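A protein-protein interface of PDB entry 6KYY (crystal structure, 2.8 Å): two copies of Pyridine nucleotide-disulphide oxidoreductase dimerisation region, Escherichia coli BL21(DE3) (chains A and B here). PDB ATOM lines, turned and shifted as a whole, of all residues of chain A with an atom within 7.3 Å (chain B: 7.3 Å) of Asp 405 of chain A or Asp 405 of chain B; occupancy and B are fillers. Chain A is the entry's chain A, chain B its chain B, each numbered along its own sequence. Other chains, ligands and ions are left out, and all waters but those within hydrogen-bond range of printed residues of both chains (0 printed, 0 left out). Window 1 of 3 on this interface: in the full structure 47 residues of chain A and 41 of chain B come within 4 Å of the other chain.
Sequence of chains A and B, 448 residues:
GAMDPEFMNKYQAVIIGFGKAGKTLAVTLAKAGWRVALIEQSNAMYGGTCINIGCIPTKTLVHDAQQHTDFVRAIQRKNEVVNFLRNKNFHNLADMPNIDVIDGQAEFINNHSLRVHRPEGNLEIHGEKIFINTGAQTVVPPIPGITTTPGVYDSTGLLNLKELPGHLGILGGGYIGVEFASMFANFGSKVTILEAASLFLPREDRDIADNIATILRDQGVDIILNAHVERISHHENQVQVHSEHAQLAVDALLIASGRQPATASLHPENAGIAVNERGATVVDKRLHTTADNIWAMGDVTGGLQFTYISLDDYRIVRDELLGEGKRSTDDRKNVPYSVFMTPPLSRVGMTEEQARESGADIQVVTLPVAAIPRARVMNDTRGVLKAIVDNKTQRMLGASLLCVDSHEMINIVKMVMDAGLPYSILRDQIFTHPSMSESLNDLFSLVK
Arg 374 of chain A touches His 407 of chain B, and with the chains exchanged His 407 of chain A touches Arg 374 of chain B. Asp 405 of chain B touches its own counterpart, Asp 405 of chain A. Glu 408 of chain A touches Arg 374 of chain B, but with the chains exchanged Arg 374 of chain A does not touch Glu 408 of chain B (4.7 Å). Glu 408 of chain A touches Ser 437 of chain B, and with the chains exchanged Ser 437 of chain A touches Glu 408 of chain B.
The side-chain hydroxyl of Ser 346 of chain A sits close to the backbone NH of His 407 of chain A (3.2 Å). SD of Met 378 of chain A is in hydrogen-bond range of NE of Arg 374 of chain A (3.4 Å). OE1 of Glu 408 of chain A sits close to NE2 of His 407 of chain A (3.4 Å). The side-chain hydroxyl of Ser 346 of chain B is in hydrogen-bond range of the backbone NH of His 407 of chain B, 3.1 Å away. NH1 of Arg 374 of chain B sits at hydrogen-bond distance from SD of Met 378 of chain B.
The guanidinium group of Arg 374 of chain A lies within hydrogen-bond range of a ring nitrogen (NE2) of His 407 of chain B (3.1 Å). NE2 of His 407 of chain A sits at hydrogen-bond distance from NH2 of Arg 374 of chain B, at 2.8 Å. The side-chain carboxylate (OE1) of Glu 408 of chain A is in salt-bridge range of the guanidinium group (NH2) of Arg 374 of chain B. The backbone NH of Met 436 of chain B sits at hydrogen-bond distance from the side-chain carboxylate of Glu 408 of chain A (2.9 Å). The side-chain carboxylate (OE2) of Glu 408 of chain A is in hydrogen-bond range of the side-chain hydroxyl (OG) of Ser 437 of chain B, at 2.4 Å. N of Met 436 of chain A sits at hydrogen-bond distance from OE2 of Glu 408 of chain B (2.8 Å). The backbone NH (N) of Ser 437 of chain A is in hydrogen-bond range of the side-chain carboxylate (OE1) of Glu 408 of chain B, at 2.9 Å. The side-chain carboxylate (OD1) of Asp 405 of chain B sits close to the side-chain carboxylate (OD1) of Asp 405 of chain A (3.3 Å).
Of the 17 printed residues of chain A, 7 touch a printed residue of chain B. Printed residues of chain A that touch a printed residue of chain B: Arg 374, Asp 405, His 407, Glu 408, Ser 435, Met 436 and Ser 437. Hydrophobic or aromatic side chains of chain A that line the printed part of chain B: His 407 and Met 436. Hydrophobic or aromatic side chains of chain B within 4 Å of the printed part of chain A: His 407 and Met 436. Among the printed residues, 9 pairs touch across the chains. Among the printed residues, Asp or Glu carboxylates within 4 Å of a Lys or Arg side-chain nitrogen of the other chain: Glu 408 of chain A with Arg 374 of chain B.
Among the printed residues, merely in contact across the chains: Ser 435 of chain A with Glu 408 of chain B.
Of the printed residues of chain B, Glu 408 of chain A touches Arg 374, Met 436 and Ser 437. Printed residues of chain A within 4 Å of Arg 374 of chain B: His 407 and Glu 408. Of chain A, only Asp 405 (3.3 Å) comes within 4 Å of Asp 405 of chain B. Of the printed residues of chain A, Ser 437 of chain B touches Glu 408. The nearest residue of chain B that does not touch Asp 405 of chain A is Glu 408 of chain B (4.03 Å).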
ATOM      1  N   PRO A 343      11.040  14.644  17.176  1.00  0.00           N
ATOM      2  CA  PRO A 343      10.482  13.975  18.357  1.00  0.00           C
ATOM      3  C   PRO A 343       9.510  12.852  17.991  1.00  0.00           C
ATOM      4  O   PRO A 343       8.900  12.903  16.924  1.00  0.00           O
ATOM      5  CB  PRO A 343       9.760  15.111  19.083  1.00  0.00           C
ATOM      6  CG  PRO A 343       9.330  16.023  17.990  1.00  0.00           C
ATOM      7  CD  PRO A 343      10.378  15.934  16.910  1.00  0.00           C
ATOM      8  N   PRO A 344       9.370  11.856  18.867  1.00  0.00           N
ATOM      9  CA  PRO A 344       8.552  10.687  18.521  1.00  0.00           C
ATOM     10  C   PRO A 344       7.068  11.020  18.469  1.00  0.00           C
ATOM     11  O   PRO A 344       6.564  11.831  19.249  1.00  0.00           O
ATOM     12  CB  PRO A 344       8.858   9.692  19.646  1.00  0.00           C
ATOM     13  CG  PRO A 344       9.309  10.535  20.787  1.00  0.00           C
ATOM     14  CD  PRO A 344      10.000  11.725  20.192  1.00  0.00           C
ATOM     15  N   SER A 346       3.476   9.531  19.113  1.00  0.00           N
ATOM     16  CA  SER A 346       2.715   8.497  19.792  1.00  0.00           C
ATOM     17  C   SER A 346       1.238   8.686  19.490  1.00  0.00           C
ATOM     18  O   SER A 346       0.759   9.819  19.385  1.00  0.00           O
ATOM     19  CB  SER A 346       2.950   8.536  21.300  1.00  0.00           C
ATOM     20  OG  SER A 346       4.052   7.725  21.644  1.00  0.00           O
ATOM     21  N   ARG A 374       8.541  22.042  29.735  1.00  0.00           N
ATOM     22  CA  ARG A 374       9.442  20.898  29.832  1.00  0.00           C
ATOM     23  C   ARG A 374      10.130  20.624  28.501  1.00  0.00           C
ATOM     24  O   ARG A 374      11.301  20.227  28.467  1.00  0.00           O
ATOM     25  CB  ARG A 374       8.676  19.666  30.312  1.00  0.00           C
ATOM     26  CG  ARG A 374       9.461  18.364  30.240  1.00  0.00           C
ATOM     27  CD  ARG A 374      10.644  18.358  31.193  1.00  0.00           C
ATOM     28  NE  ARG A 374      11.410  17.120  31.083  1.00  0.00           N
ATOM     29  CZ  ARG A 374      12.460  16.819  31.839  1.00  0.00           C
ATOM     30  NH1 ARG A 374      13.094  15.668  31.664  1.00  0.00           N
ATOM     31  NH2 ARG A 374      12.876  17.667  32.770  1.00  0.00           N
ATOM     32  N   MET A 378      14.327  20.480  27.612  1.00  0.00           N
ATOM     33  CA  MET A 378      15.017  19.423  26.889  1.00  0.00           C
ATOM     34  C   MET A 378      15.495  19.859  25.509  1.00  0.00           C
ATOM     35  O   MET A 378      15.931  19.011  24.723  1.00  0.00           O
ATOM     36  CB  MET A 378      14.111  18.200  26.763  1.00  0.00           C
ATOM     37  CG  MET A 378      13.438  17.807  28.064  1.00  0.00           C
ATOM     38  SD  MET A 378      12.371  16.376  27.860  1.00  0.00           S
ATOM     39  CE  MET A 378      13.569  15.054  27.992  1.00  0.00           C
ATOM     40  N   LEU A 401       0.161  12.626  19.948  1.00  0.00           N
ATOM     41  CA  LEU A 401       1.150  13.338  20.751  1.00  0.00           C
ATOM     42  C   LEU A 401       2.482  13.300  20.008  1.00  0.00           C
ATOM     43  O   LEU A 401       3.162  12.271  19.984  1.00  0.00           O
ATOM     44  CB  LEU A 401       1.261  12.719  22.142  1.00  0.00           C
ATOM     45  CG  LEU A 401      -0.042  12.691  22.947  1.00  0.00           C
ATOM     46  CD1 LEU A 401       0.206  12.238  24.377  1.00  0.00           C
ATOM     47  CD2 LEU A 401      -0.716  14.053  22.924  1.00  0.00           C
ATOM     48  N   CYS A 403       5.751  14.902  20.415  1.00  0.00           N
ATOM     49  CA  CYS A 403       6.557  15.672  21.351  1.00  0.00           C
ATOM     50  C   CYS A 403       7.617  14.760  21.949  1.00  0.00           C
ATOM     51  O   CYS A 403       7.596  13.541  21.760  1.00  0.00           O
ATOM     52  CB  CYS A 403       5.688  16.286  22.453  1.00  0.00           C
ATOM     53  SG  CYS A 403       4.858  15.061  23.493  1.00  0.00           S
ATOM     54  N   VAL A 404       8.551  15.372  22.675  1.00  0.00           N
ATOM     55  CA  VAL A 404       9.553  14.601  23.398  1.00  0.00           C
ATOM     56  C   VAL A 404       8.872  13.804  24.503  1.00  0.00           C
ATOM     57  O   VAL A 404       7.966  14.301  25.187  1.00  0.00           O
ATOM     58  CB  VAL A 404      10.650  15.531  23.952  1.00  0.00           C
ATOM     59  CG1 VAL A 404      10.048  16.620  24.833  1.00  0.00           C
ATOM     60  CG2 VAL A 404      11.700  14.734  24.711  1.00  0.00           C
ATOM     61  N   ASP A 405       9.286  12.544  24.658  1.00  0.00           N
ATOM     62  CA  ASP A 405       8.729  11.629  25.656  1.00  0.00           C
ATOM     63  C   ASP A 405       7.242  11.362  25.422  1.00  0.00           C
ATOM     64  O   ASP A 405       6.498  11.073  26.363  1.00  0.00           O
ATOM     65  CB  ASP A 405       8.962  12.142  27.080  1.00  0.00           C
ATOM     66  CG  ASP A 405      10.395  11.970  27.534  1.00  0.00           C
ATOM     67  OD1 ASP A 405      10.877  12.810  28.323  1.00  0.00           O
ATOM     68  OD2 ASP A 405      11.040  10.991  27.102  1.00  0.00           O
ATOM     69  N   SER A 406       6.798  11.453  24.167  1.00  0.00           N
ATOM     70  CA  SER A 406       5.408  11.138  23.853  1.00  0.00           C
ATOM     71  C   SER A 406       5.120   9.652  24.014  1.00  0.00           C
ATOM     72  O   SER A 406       3.986   9.270  24.320  1.00  0.00           O
ATOM     73  CB  SER A 406       5.073  11.591  22.433  1.00  0.00           C
ATOM     74  OG  SER A 406       5.446  10.606  21.484  1.00  0.00           O
ATOM     75  N   HIS A 407       6.132   8.805  23.812  1.00  0.00           N
ATOM     76  CA  HIS A 407       5.966   7.368  23.990  1.00  0.00           C
ATOM     77  C   HIS A 407       5.660   6.994  25.433  1.00  0.00           C
ATOM     78  O   HIS A 407       5.103   5.919  25.678  1.00  0.00           O
ATOM     79  CB  HIS A 407       7.225   6.639  23.521  1.00  0.00           C
ATOM     80  CG  HIS A 407       8.466   7.074  24.234  1.00  0.00           C
ATOM     81  ND1 HIS A 407       8.976   8.350  24.129  1.00  0.00           N
ATOM     82  CD2 HIS A 407       9.293   6.406  25.073  1.00  0.00           C
ATOM     83  CE1 HIS A 407      10.066   8.448  24.867  1.00  0.00           C
ATOM     84  NE2 HIS A 407      10.280   7.284  25.451  1.00  0.00           N
ATOM     85  N   GLU A 408       6.009   7.854  26.389  1.00  0.00           N
ATOM     86  CA  GLU A 408       5.761   7.573  27.796  1.00  0.00           C
ATOM     87  C   GLU A 408       4.429   8.133  28.276  1.00  0.00           C
ATOM     88  O   GLU A 408       3.725   7.473  29.048  1.00  0.00           O
ATOM     89  CB  GLU A 408       6.899   8.136  28.652  1.00  0.00           C
ATOM     90  CG  GLU A 408       8.276   7.608  28.284  1.00  0.00           C
ATOM     91  CD  GLU A 408       8.489   6.175  28.728  1.00  0.00           C
ATOM     92  OE1 GLU A 408       9.296   5.467  28.092  1.00  0.00           O
ATOM     93  OE2 GLU A 408       7.851   5.755  29.715  1.00  0.00           O
ATOM     94  N   MET A 409       4.062   9.335  27.831  1.00  0.00           N
ATOM     95  CA  MET A 409       2.855   9.996  28.308  1.00  0.00           C
ATOM     96  C   MET A 409       1.595   9.558  27.572  1.00  0.00           C
ATOM     97  O   MET A 409       0.491   9.875  28.028  1.00  0.00           O
ATOM     98  CB  MET A 409       3.008  11.517  28.205  1.00  0.00           C
ATOM     99  CG  MET A 409       2.941  12.059  26.790  1.00  0.00           C
ATOM    100  SD  MET A 409       3.647  13.713  26.653  1.00  0.00           S
ATOM    101  CE  MET A 409       2.166  14.702  26.457  1.00  0.00           C
ATOM    102  N   ILE A 410       1.726   8.844  26.450  1.00  0.00           N
ATOM    103  CA  ILE A 410       0.552   8.301  25.779  1.00  0.00           C
ATOM    104  C   ILE A 410      -0.028   7.122  26.549  1.00  0.00           C
ATOM    105  O   ILE A 410      -1.221   6.823  26.416  1.00  0.00           O
ATOM    106  CB  ILE A 410       0.896   7.899  24.332  1.00  0.00           C
ATOM    107  CG1 ILE A 410      -0.378   7.693  23.509  1.00  0.00           C
ATOM    108  CG2 ILE A 410       1.767   6.652  24.311  1.00  0.00           C
ATOM    109  CD1 ILE A 410      -0.885   8.952  22.844  1.00  0.00           C
ATOM    110  N   SER A 435       7.383  18.090  33.904  1.00  0.00           N
ATOM    111  CA  SER A 435       7.253  16.869  33.128  1.00  0.00           C
ATOM    112  C   SER A 435       6.590  17.178  31.793  1.00  0.00           C
ATOM    113  O   SER A 435       6.112  18.289  31.548  1.00  0.00           O
ATOM    114  CB  SER A 435       6.439  15.810  33.885  1.00  0.00           C
ATOM    115  OG  SER A 435       5.164  16.312  34.245  1.00  0.00           O
ATOM    116  N   MET A 436       6.577  16.172  30.919  1.00  0.00           N
ATOM    117  CA  MET A 436       5.801  16.247  29.688  1.00  0.00           C
ATOM    118  C   MET A 436       4.367  15.780  29.886  1.00  0.00           C
ATOM    119  O   MET A 436       3.467  16.249  29.183  1.00  0.00           O
ATOM    120  CB  MET A 436       6.465  15.414  28.589  1.00  0.00           C
ATOM    121  CG  MET A 436       7.732  16.030  28.023  1.00  0.00           C
ATOM    122  SD  MET A 436       7.480  17.714  27.434  1.00  0.00           S
ATOM    123  CE  MET A 436       6.597  17.416  25.906  1.00  0.00           C
ATOM    124  N   SER A 437       4.138  14.868  30.836  1.00  0.00           N
ATOM    125  CA  SER A 437       2.785  14.422  31.140  1.00  0.00           C
ATOM    126  C   SER A 437       1.930  15.533  31.730  1.00  0.00           C
ATOM    127  O   SER A 437       0.699  15.463  31.644  1.00  0.00           O
ATOM    128  CB  SER A 437       2.823  13.237  32.106  1.00  0.00           C
ATOM    129  OG  SER A 437       3.929  12.392  31.841  1.00  0.00           O
ATOM    130  N   PRO B 343      19.960   8.786  37.699  1.00  0.00           N
ATOM    131  CA  PRO B 343      18.560   8.878  37.272  1.00  0.00           C
ATOM    132  C   PRO B 343      17.640   9.458  38.347  1.00  0.00           C
ATOM    133  O   PRO B 343      17.916   9.305  39.536  1.00  0.00           O
ATOM    134  CB  PRO B 343      18.202   7.424  36.978  1.00  0.00           C
ATOM    135  CG  PRO B 343      19.031   6.648  37.942  1.00  0.00           C
ATOM    136  CD  PRO B 343      20.301   7.431  38.168  1.00  0.00           C
ATOM    137  N   PRO B 344      16.563  10.119  37.928  1.00  0.00           N
ATOM    138  CA  PRO B 344      15.679  10.781  38.896  1.00  0.00           C
ATOM    139  C   PRO B 344      14.914   9.791  39.766  1.00  0.00           C
ATOM    140  O   PRO B 344      14.611   8.667  39.359  1.00  0.00           O
ATOM    141  CB  PRO B 344      14.728  11.599  38.015  1.00  0.00           C
ATOM    142  CG  PRO B 344      14.854  11.017  36.641  1.00  0.00           C
ATOM    143  CD  PRO B 344      16.233  10.464  36.535  1.00  0.00           C
ATOM    144  N   SER B 346      11.491   9.203  41.671  1.00  0.00           N
ATOM    145  CA  SER B 346      10.088   9.578  41.745  1.00  0.00           C
ATOM    146  C   SER B 346       9.359   8.673  42.729  1.00  0.00           C
ATOM    147  O   SER B 346       9.682   7.490  42.865  1.00  0.00           O
ATOM    148  CB  SER B 346       9.427   9.501  40.368  1.00  0.00           C
ATOM    149  OG  SER B 346       9.953  10.493  39.507  1.00  0.00           O
ATOM    150  N   ARG B 374      14.798  -0.632  27.916  1.00  0.00           N
ATOM    151  CA  ARG B 374      14.807   0.758  27.474  1.00  0.00           C
ATOM    152  C   ARG B 374      15.842   1.582  28.232  1.00  0.00           C
ATOM    153  O   ARG B 374      16.381   2.552  27.685  1.00  0.00           O
ATOM    154  CB  ARG B 374      13.415   1.367  27.630  1.00  0.00           C
ATOM    155  CG  ARG B 374      13.327   2.828  27.226  1.00  0.00           C
ATOM    156  CD  ARG B 374      13.123   2.985  25.725  1.00  0.00           C
ATOM    157  NE  ARG B 374      13.759   4.187  25.187  1.00  0.00           N
ATOM    158  CZ  ARG B 374      13.407   5.432  25.497  1.00  0.00           C
ATOM    159  NH1 ARG B 374      14.049   6.456  24.951  1.00  0.00           N
ATOM    160  NH2 ARG B 374      12.417   5.660  26.349  1.00  0.00           N
ATOM    161  N   MET B 378      19.063   3.850  26.521  1.00  0.00           N
ATOM    162  CA  MET B 378      19.411   5.230  26.825  1.00  0.00           C
ATOM    163  C   MET B 378      20.746   5.365  27.551  1.00  0.00           C
ATOM    164  O   MET B 378      21.076   6.463  28.014  1.00  0.00           O
ATOM    165  CB  MET B 378      18.297   5.878  27.649  1.00  0.00           C
ATOM    166  CG  MET B 378      16.939   5.836  26.975  1.00  0.00           C
ATOM    167  SD  MET B 378      15.807   7.087  27.605  1.00  0.00           S
ATOM    168  CE  MET B 378      14.972   6.164  28.890  1.00  0.00           C
ATOM    169  N   LEU B 401      10.313   4.771  42.254  1.00  0.00           N
ATOM    170  CA  LEU B 401      10.763   4.656  40.872  1.00  0.00           C
ATOM    171  C   LEU B 401      12.062   5.443  40.726  1.00  0.00           C
ATOM    172  O   LEU B 401      12.044   6.661  40.530  1.00  0.00           O
ATOM    173  CB  LEU B 401       9.680   5.149  39.919  1.00  0.00           C
ATOM    174  CG  LEU B 401       8.371   4.360  40.020  1.00  0.00           C
ATOM    175  CD1 LEU B 401       7.425   4.715  38.887  1.00  0.00           C
ATOM    176  CD2 LEU B 401       8.638   2.861  40.039  1.00  0.00           C
ATOM    177  N   CYS B 403      14.671   5.631  38.293  1.00  0.00           N
ATOM    178  CA  CYS B 403      14.999   5.259  36.927  1.00  0.00           C
ATOM    179  C   CYS B 403      15.056   6.513  36.071  1.00  0.00           C
ATOM    180  O   CYS B 403      14.653   7.600  36.494  1.00  0.00           O
ATOM    181  CB  CYS B 403      13.972   4.277  36.365  1.00  0.00           C
ATOM    182  SG  CYS B 403      12.286   4.699  36.819  1.00  0.00           S
ATOM    183  N   VAL B 404      15.567   6.350  34.852  1.00  0.00           N
ATOM    184  CA  VAL B 404      15.456   7.407  33.861  1.00  0.00           C
ATOM    185  C   VAL B 404      13.991   7.570  33.478  1.00  0.00           C
ATOM    186  O   VAL B 404      13.249   6.585  33.361  1.00  0.00           O
ATOM    187  CB  VAL B 404      16.329   7.094  32.634  1.00  0.00           C
ATOM    188  CG1 VAL B 404      17.771   7.500  32.895  1.00  0.00           C
ATOM    189  CG2 VAL B 404      16.243   5.617  32.289  1.00  0.00           C
ATOM    190  N   ASP B 405      13.565   8.822  33.302  1.00  0.00           N
ATOM    191  CA  ASP B 405      12.171   9.157  33.003  1.00  0.00           C
ATOM    192  C   ASP B 405      11.227   8.715  34.119  1.00  0.00           C
ATOM    193  O   ASP B 405      10.058   8.411  33.874  1.00  0.00           O
ATOM    194  CB  ASP B 405      11.727   8.566  31.662  1.00  0.00           C
ATOM    195  CG  ASP B 405      12.119   9.436  30.487  1.00  0.00           C
ATOM    196  OD1 ASP B 405      12.018  10.675  30.608  1.00  0.00           O
ATOM    197  OD2 ASP B 405      12.530   8.883  29.446  1.00  0.00           O
ATOM    198  N   SER B 406      11.726   8.682  35.357  1.00  0.00           N
ATOM    199  CA  SER B 406      10.866   8.338  36.484  1.00  0.00           C
ATOM    200  C   SER B 406       9.789   9.391  36.708  1.00  0.00           C
ATOM    201  O   SER B 406       8.696   9.069  37.189  1.00  0.00           O
ATOM    202  CB  SER B 406      11.704   8.169  37.749  1.00  0.00           C
ATOM    203  OG  SER B 406      12.559   9.281  37.940  1.00  0.00           O
ATOM    204  N   HIS B 407      10.074  10.649  36.365  1.00  0.00           N
ATOM    205  CA  HIS B 407       9.145  11.749  36.594  1.00  0.00           C
ATOM    206  C   HIS B 407       7.881  11.656  35.749  1.00  0.00           C
ATOM    207  O   HIS B 407       6.912  12.367  36.041  1.00  0.00           O
ATOM    208  CB  HIS B 407       9.845  13.082  36.323  1.00  0.00           C
ATOM    209  CG  HIS B 407      10.484  13.164  34.971  1.00  0.00           C
ATOM    210  ND1 HIS B 407      11.560  12.384  34.606  1.00  0.00           N
ATOM    211  CD2 HIS B 407      10.195  13.932  33.894  1.00  0.00           C
ATOM    212  CE1 HIS B 407      11.906  12.667  33.364  1.00  0.00           C
ATOM    213  NE2 HIS B 407      11.094  13.604  32.909  1.00  0.00           N
ATOM    214  N   GLU B 408       7.861  10.811  34.718  1.00  0.00           N
ATOM    215  CA  GLU B 408       6.689  10.649  33.867  1.00  0.00           C
ATOM    216  C   GLU B 408       5.841   9.446  34.259  1.00  0.00           C
ATOM    217  O   GLU B 408       4.636   9.584  34.489  1.00  0.00           O
ATOM    218  CB  GLU B 408       7.114  10.525  32.398  1.00  0.00           C
ATOM    219  CG  GLU B 408       8.094  11.593  31.934  1.00  0.00           C
ATOM    220  CD  GLU B 408       7.415  12.901  31.577  1.00  0.00           C
ATOM    221  OE1 GLU B 408       6.192  13.027  31.800  1.00  0.00           O
ATOM    222  OE2 GLU B 408       8.108  13.807  31.069  1.00  0.00           O
ATOM    223  N   MET B 409       6.451   8.263  34.348  1.00  0.00           N
ATOM    224  CA  MET B 409       5.691   7.052  34.631  1.00  0.00           C
ATOM    225  C   MET B 409       5.178   7.003  36.065  1.00  0.00           C
ATOM    226  O   MET B 409       4.283   6.202  36.358  1.00  0.00           O
ATOM    227  CB  MET B 409       6.545   5.819  34.342  1.00  0.00           C
ATOM    228  CG  MET B 409       7.549   5.500  35.428  1.00  0.00           C
ATOM    229  SD  MET B 409       8.738   4.250  34.917  1.00  0.00           S
ATOM    230  CE  MET B 409      10.043   5.310  34.320  1.00  0.00           C
ATOM    231  N   ILE B 410       5.718   7.831  36.963  1.00  0.00           N
ATOM    232  CA  ILE B 410       5.183   7.890  38.320  1.00  0.00           C
ATOM    233  C   ILE B 410       3.750   8.404  38.305  1.00  0.00           C
ATOM    234  O   ILE B 410       2.951   8.070  39.188  1.00  0.00           O
ATOM    235  CB  ILE B 410       6.089   8.753  39.223  1.00  0.00           C
ATOM    236  CG1 ILE B 410       5.696   8.597  40.695  1.00  0.00           C
ATOM    237  CG2 ILE B 410       6.037  10.215  38.807  1.00  0.00           C
ATOM    238  CD1 ILE B 410       6.003   7.233  41.270  1.00  0.00           C
ATOM    239  N   MET B 436       9.996   2.991  29.325  1.00  0.00           N
ATOM    240  CA  MET B 436      10.256   2.757  30.736  1.00  0.00           C
ATOM    241  C   MET B 436       8.977   2.491  31.513  1.00  0.00           C
ATOM    242  O   MET B 436       9.017   1.827  32.555  1.00  0.00           O
ATOM    243  CB  MET B 436      10.997   3.952  31.340  1.00  0.00           C
ATOM    244  CG  MET B 436      12.310   4.277  30.664  1.00  0.00           C
ATOM    245  SD  MET B 436      13.505   2.948  30.856  1.00  0.00           S
ATOM    246  CE  MET B 436      13.684   2.901  32.632  1.00  0.00           C
ATOM    247  N   SER B 437       7.841   2.989  31.019  1.00  0.00           N
ATOM    248  CA  SER B 437       6.564   2.702  31.661  1.00  0.00           C
ATOM    249  C   SER B 437       6.170   1.242  31.492  1.00  0.00           C
ATOM    250  O   SER B 437       5.465   0.688  32.342  1.00  0.00           O
ATOM    251  CB  SER B 437       5.476   3.613  31.093  1.00  0.00           C
ATOM    252  OG  SER B 437       5.943   4.944  30.955  1.00  0.00           O
